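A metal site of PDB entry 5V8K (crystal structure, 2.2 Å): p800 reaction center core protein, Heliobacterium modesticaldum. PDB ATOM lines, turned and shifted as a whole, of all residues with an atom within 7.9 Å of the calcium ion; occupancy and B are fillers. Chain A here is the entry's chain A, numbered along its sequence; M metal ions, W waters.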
ATOM      1  N   ILE A 251      -8.946  26.478   0.628  1.00  0.00           N
ATOM      2  CA  ILE A 251      -8.534  26.890   1.971  1.00  0.00           C
ATOM      3  C   ILE A 251      -7.131  26.386   2.277  1.00  0.00           C
ATOM      4  O   ILE A 251      -6.265  27.136   2.747  1.00  0.00           O
ATOM      5  CB  ILE A 251      -9.557  26.400   3.014  1.00  0.00           C
ATOM      6  CG1 ILE A 251     -10.887  27.150   2.828  1.00  0.00           C
ATOM      7  CG2 ILE A 251      -9.057  26.612   4.417  1.00  0.00           C
ATOM      8  CD1 ILE A 251     -12.043  26.543   3.569  1.00  0.00           C
ATOM      9  N   ASN A 255      -3.564  27.845   3.564  1.00  0.00           N
ATOM     10  CA  ASN A 255      -3.417  27.352   4.939  1.00  0.00           C
ATOM     11  C   ASN A 255      -3.108  25.874   4.888  1.00  0.00           C
ATOM     12  O   ASN A 255      -3.964  25.031   5.206  1.00  0.00           O
ATOM     13  CB  ASN A 255      -4.670  27.636   5.758  1.00  0.00           C
ATOM     14  CG  ASN A 255      -4.493  27.327   7.199  1.00  0.00           C
ATOM     15  OD1 ASN A 255      -3.456  26.834   7.654  1.00  0.00           O
ATOM     16  ND2 ASN A 255      -5.536  27.561   7.953  1.00  0.00           N
ATOM     17  N   LEU A 258      -4.077  23.237   7.608  1.00  0.00           N
ATOM     18  CA  LEU A 258      -5.450  23.358   8.081  1.00  0.00           C
ATOM     19  C   LEU A 258      -5.879  22.168   8.922  1.00  0.00           C
ATOM     20  O   LEU A 258      -6.239  22.322  10.095  1.00  0.00           O
ATOM     21  CB  LEU A 258      -6.413  23.529   6.895  1.00  0.00           C
ATOM     22  CG  LEU A 258      -7.896  23.708   7.235  1.00  0.00           C
ATOM     23  CD1 LEU A 258      -8.200  25.088   7.810  1.00  0.00           C
ATOM     24  CD2 LEU A 258      -8.726  23.444   5.983  1.00  0.00           C
ATOM     25  N   LYS A 261      -3.739  21.198  12.060  1.00  0.00           N
ATOM     26  CA  LYS A 261      -3.972  22.045  13.226  1.00  0.00           C
ATOM     27  C   LYS A 261      -5.339  21.801  13.868  1.00  0.00           C
ATOM     28  O   LYS A 261      -5.462  22.009  15.082  1.00  0.00           O
ATOM     29  CB  LYS A 261      -3.775  23.502  12.848  1.00  0.00           C
ATOM     30  CG  LYS A 261      -2.341  23.777  12.582  1.00  0.00           C
ATOM     31  CD  LYS A 261      -2.063  25.188  12.159  1.00  0.00           C
ATOM     32  CE  LYS A 261      -2.549  25.455  10.791  1.00  0.00           C
ATOM     33  NZ  LYS A 261      -2.313  26.849  10.383  1.00  0.00           N
ATOM     34  N   TRP A 456      -2.565  27.864  21.033  1.00  0.00           N
ATOM     35  CA  TRP A 456      -3.256  27.903  19.752  1.00  0.00           C
ATOM     36  C   TRP A 456      -2.808  29.099  18.919  1.00  0.00           C
ATOM     37  O   TRP A 456      -2.493  28.955  17.725  1.00  0.00           O
ATOM     38  CB  TRP A 456      -4.785  27.941  19.949  1.00  0.00           C
ATOM     39  CG  TRP A 456      -5.415  28.196  18.601  1.00  0.00           C
ATOM     40  CD1 TRP A 456      -5.973  29.354  18.197  1.00  0.00           C
ATOM     41  CD2 TRP A 456      -5.445  27.312  17.479  1.00  0.00           C
ATOM     42  NE1 TRP A 456      -6.357  29.256  16.874  1.00  0.00           N
ATOM     43  CE2 TRP A 456      -6.039  28.011  16.400  1.00  0.00           C
ATOM     44  CE3 TRP A 456      -5.008  26.005  17.258  1.00  0.00           C
ATOM     45  CZ2 TRP A 456      -6.233  27.437  15.122  1.00  0.00           C
ATOM     46  CZ3 TRP A 456      -5.188  25.432  15.984  1.00  0.00           C
ATOM     47  CH2 TRP A 456      -5.809  26.145  14.946  1.00  0.00           C
ATOM     48  N   ASP A 460      -1.053  28.577  15.236  1.00  0.00           N
ATOM     49  CA  ASP A 460      -1.656  29.116  14.039  1.00  0.00           C
ATOM     50  C   ASP A 460      -0.879  30.290  13.445  1.00  0.00           C
ATOM     51  O   ASP A 460      -1.428  30.979  12.593  1.00  0.00           O
ATOM     52  CB  ASP A 460      -3.089  29.575  14.297  1.00  0.00           C
ATOM     53  CG  ASP A 460      -4.038  29.209  13.131  1.00  0.00           C
ATOM     54  OD1 ASP A 460      -3.759  28.249  12.399  1.00  0.00           O
ATOM     55  OD2 ASP A 460      -5.038  29.922  12.951  1.00  0.00           O
ATOM     56  N   GLY A 461       0.359  30.542  13.865  1.00  0.00           N
ATOM     57  CA  GLY A 461       1.174  31.548  13.196  1.00  0.00           C
ATOM     58  C   GLY A 461       0.959  32.997  13.611  1.00  0.00           C
ATOM     59  O   GLY A 461       1.390  33.892  12.874  1.00  0.00           O
ATOM     60  N   SER A 495       1.944  26.503   9.204  1.00  0.00           N
ATOM     61  CA  SER A 495       1.494  27.871   9.364  1.00  0.00           C
ATOM     62  C   SER A 495       2.592  28.832   8.892  1.00  0.00           C
ATOM     63  O   SER A 495       3.752  28.670   9.290  1.00  0.00           O
ATOM     64  CB  SER A 495       1.151  28.179  10.829  1.00  0.00           C
ATOM     65  OG  SER A 495       0.208  27.270  11.351  1.00  0.00           O
ATOM     66  N   TYR A 505      -4.982  39.296  14.561  1.00  0.00           N
ATOM     67  CA  TYR A 505      -5.270  38.021  13.917  1.00  0.00           C
ATOM     68  C   TYR A 505      -6.746  37.669  14.049  1.00  0.00           C
ATOM     69  O   TYR A 505      -7.352  37.117  13.128  1.00  0.00           O
ATOM     70  CB  TYR A 505      -4.346  36.941  14.503  1.00  0.00           C
ATOM     71  CG  TYR A 505      -4.803  35.495  14.505  1.00  0.00           C
ATOM     72  CD1 TYR A 505      -5.605  35.025  15.520  1.00  0.00           C
ATOM     73  CD2 TYR A 505      -4.331  34.585  13.583  1.00  0.00           C
ATOM     74  CE1 TYR A 505      -5.989  33.705  15.594  1.00  0.00           C
ATOM     75  CE2 TYR A 505      -4.713  33.267  13.626  1.00  0.00           C
ATOM     76  CZ  TYR A 505      -5.551  32.817  14.637  1.00  0.00           C
ATOM     77  OH  TYR A 505      -5.959  31.485  14.721  1.00  0.00           O
ATOM     78  N   GLN A 508      -8.566  39.531  11.304  1.00  0.00           N
ATOM     79  CA  GLN A 508      -8.335  38.980   9.980  1.00  0.00           C
ATOM     80  C   GLN A 508      -9.017  37.613   9.791  1.00  0.00           C
ATOM     81  O   GLN A 508      -9.630  37.366   8.758  1.00  0.00           O
ATOM     82  CB  GLN A 508      -6.831  38.870   9.743  1.00  0.00           C
ATOM     83  CG  GLN A 508      -6.452  38.438   8.336  1.00  0.00           C
ATOM     84  CD  GLN A 508      -6.470  36.925   8.171  1.00  0.00           C
ATOM     85  OE1 GLN A 508      -6.143  36.169   9.081  1.00  0.00           O
ATOM     86  NE2 GLN A 508      -6.815  36.483   6.979  1.00  0.00           N
ATOM     87  N   GLN A 509      -8.911  36.732  10.783  1.00  0.00           N
ATOM     88  CA  GLN A 509      -9.551  35.426  10.724  1.00  0.00           C
ATOM     89  C   GLN A 509     -11.076  35.558  10.701  1.00  0.00           C
ATOM     90  O   GLN A 509     -11.752  34.927   9.877  1.00  0.00           O
ATOM     91  CB  GLN A 509      -9.098  34.586  11.892  1.00  0.00           C
ATOM     92  CG  GLN A 509      -7.635  34.147  11.834  1.00  0.00           C
ATOM     93  CD  GLN A 509      -7.387  32.989  10.933  1.00  0.00           C
ATOM     94  OE1 GLN A 509      -7.605  31.822  11.297  1.00  0.00           O
ATOM     95  NE2 GLN A 509      -6.916  33.285   9.770  1.00  0.00           N
ATOM     96  N   MET A 513     -13.855  34.403   7.942  1.00  0.00           N
ATOM     97  CA  MET A 513     -14.956  33.497   8.246  1.00  0.00           C
ATOM     98  C   MET A 513     -16.231  33.860   7.498  1.00  0.00           C
ATOM     99  O   MET A 513     -17.069  32.977   7.243  1.00  0.00           O
ATOM    100  CB  MET A 513     -15.247  33.460   9.748  1.00  0.00           C
ATOM    101  CG  MET A 513     -14.245  32.720  10.561  1.00  0.00           C
ATOM    102  SD  MET A 513     -14.586  32.986  12.328  1.00  0.00           S
ATOM    103  CE  MET A 513     -12.967  32.690  13.054  1.00  0.00           C
ATOM    104  N   MET A 594     -12.456  28.936  19.264  1.00  0.00           N
ATOM    105  CA  MET A 594     -11.120  28.624  18.775  1.00  0.00           C
ATOM    106  C   MET A 594     -11.200  27.638  17.628  1.00  0.00           C
ATOM    107  O   MET A 594     -10.414  27.717  16.682  1.00  0.00           O
ATOM    108  CB  MET A 594     -10.266  28.064  19.917  1.00  0.00           C
ATOM    109  CG  MET A 594      -9.975  29.103  21.021  1.00  0.00           C
ATOM    110  SD  MET A 594      -9.006  28.357  22.311  1.00  0.00           S
ATOM    111  CE  MET A 594      -7.491  28.646  21.507  1.00  0.00           C
ATOM    112  N   TRP A 595     -12.175  26.723  17.672  1.00  0.00           N
ATOM    113  CA  TRP A 595     -12.421  25.824  16.560  1.00  0.00           C
ATOM    114  C   TRP A 595     -12.774  26.595  15.279  1.00  0.00           C
ATOM    115  O   TRP A 595     -12.277  26.278  14.202  1.00  0.00           O
ATOM    116  CB  TRP A 595     -13.513  24.838  16.939  1.00  0.00           C
ATOM    117  CG  TRP A 595     -13.527  23.762  15.924  1.00  0.00           C
ATOM    118  CD1 TRP A 595     -14.350  23.671  14.848  1.00  0.00           C
ATOM    119  CD2 TRP A 595     -12.608  22.676  15.834  1.00  0.00           C
ATOM    120  NE1 TRP A 595     -14.013  22.566  14.097  1.00  0.00           N
ATOM    121  CE2 TRP A 595     -12.948  21.926  14.688  1.00  0.00           C
ATOM    122  CE3 TRP A 595     -11.536  22.253  16.625  1.00  0.00           C
ATOM    123  CZ2 TRP A 595     -12.244  20.810  14.299  1.00  0.00           C
ATOM    124  CZ3 TRP A 595     -10.835  21.134  16.245  1.00  0.00           C
ATOM    125  CH2 TRP A 595     -11.196  20.420  15.093  1.00  0.00           C
ATOM    126  N   ALA A 596     -13.572  27.651  15.384  1.00  0.00           N
ATOM    127  CA  ALA A 596     -13.787  28.531  14.231  1.00  0.00           C
ATOM    128  C   ALA A 596     -12.488  29.029  13.637  1.00  0.00           C
ATOM    129  O   ALA A 596     -12.315  29.010  12.421  1.00  0.00           O
ATOM    130  CB  ALA A 596     -14.664  29.708  14.633  1.00  0.00           C
ATOM    131  N   LEU A 597     -11.561  29.460  14.492  1.00  0.00           N
ATOM    132  CA  LEU A 597     -10.243  29.874  14.041  1.00  0.00           C
ATOM    133  C   LEU A 597      -9.492  28.735  13.387  1.00  0.00           C
ATOM    134  O   LEU A 597      -8.661  28.984  12.507  1.00  0.00           O
ATOM    135  CB  LEU A 597      -9.388  30.434  15.220  1.00  0.00           C
ATOM    136  CG  LEU A 597      -9.871  31.690  15.911  1.00  0.00           C
ATOM    137  CD1 LEU A 597      -9.032  31.919  17.155  1.00  0.00           C
ATOM    138  CD2 LEU A 597      -9.756  32.831  14.933  1.00  0.00           C
ATOM    139  N   ALA A 598      -9.700  27.506  13.843  1.00  0.00           N
ATOM    140  CA  ALA A 598      -9.055  26.340  13.226  1.00  0.00           C
ATOM    141  C   ALA A 598      -9.689  25.935  11.888  1.00  0.00           C
ATOM    142  O   ALA A 598      -9.067  25.176  11.131  1.00  0.00           O
ATOM    143  CB  ALA A 598      -9.103  25.154  14.176  1.00  0.00           C
ATOM    144  N   MET A 599     -10.860  26.458  11.567  1.00  0.00           N
ATOM    145  CA  MET A 599     -11.564  26.095  10.341  1.00  0.00           C
ATOM    146  C   MET A 599     -11.203  26.985   9.159  1.00  0.00           C
ATOM    147  O   MET A 599     -11.457  26.585   8.005  1.00  0.00           O
ATOM    148  CB  MET A 599     -13.069  26.145  10.558  1.00  0.00           C
ATOM    149  CG  MET A 599     -13.574  24.975  11.383  1.00  0.00           C
ATOM    150  SD  MET A 599     -13.239  23.301  10.736  1.00  0.00           S
ATOM    151  CE  MET A 599     -14.526  23.173   9.483  1.00  0.00           C
ATOM    152  N   VAL A 600     -10.662  28.167   9.412  1.00  0.00           N
ATOM    153  CA  VAL A 600     -10.184  29.054   8.382  1.00  0.00           C
ATOM    154  C   VAL A 600      -8.660  29.279   8.473  1.00  0.00           C
ATOM    155  O   VAL A 600      -8.054  29.367   7.359  1.00  0.00           O
ATOM    156  CB  VAL A 600     -10.949  30.400   8.413  1.00  0.00           C
ATOM    157  CG1 VAL A 600     -12.425  30.153   8.231  1.00  0.00           C
ATOM    158  CG2 VAL A 600     -10.678  31.148   9.724  1.00  0.00           C
HETATM  159 CA    CA M   1      -6.751  29.635  11.266  1.00  0.00          CA
HETATM  160  O   HOH W   1      -5.733  27.345  11.054  1.00  0.00           O
HETATM  161  O   HOH W   2      -4.970  30.262   9.863  1.00  0.00           O
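OE1 of Gln 508 is in hydrogen-bond range of NE2 of Gln 509 (3.1 Å). OD2 of Asp 460 lies close to OH of Tyr 505 (2.5 Å). The side-chain amino group (NZ) of Lys 261 is in salt-bridge range of the side-chain carboxylate (OD1) of Asp 460 (2.8 Å). The backbone carbonyl oxygen (O) of Val 600 is in hydrogen-bond range of the side-chain amide nitrogen (ND2) of Asn 255 (3.2 Å). NE1 of Trp 456 sits at hydrogen-bond distance from OH of Tyr 505, at 3.1 Å.
Tyr 505 touches the calcium ion (OH to CA, 3.998 Å). Val 600 touches the calcium ion (C to CA, 3.4 Å). Five residues have an atom within 4 Å of the calcium ion: Asp 460, Tyr 505, Gln 509, Leu 597 and Val 600.
OE1 of Gln 509 binds the calcium ion (2.3 Å). Water W2 binds the calcium ion. The backbone carbonyl oxygen (O) of Leu 597 binds the calcium ion, 2.4 Å away. OD2 of Asp 460 is bound to the calcium ion (2.4 Å). Water W1 is bound to the calcium ion (2.5 Å). The calcium ion has five donor atoms within binding distance.
Water W2 lies within hydrogen-bond range of ND2 of Asn 255 (3.4 Å) and OD1 of Asp 460 (3.5 Å). Water W1 bridges OD1 of Asp 460 and ND2 of Asn 255.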
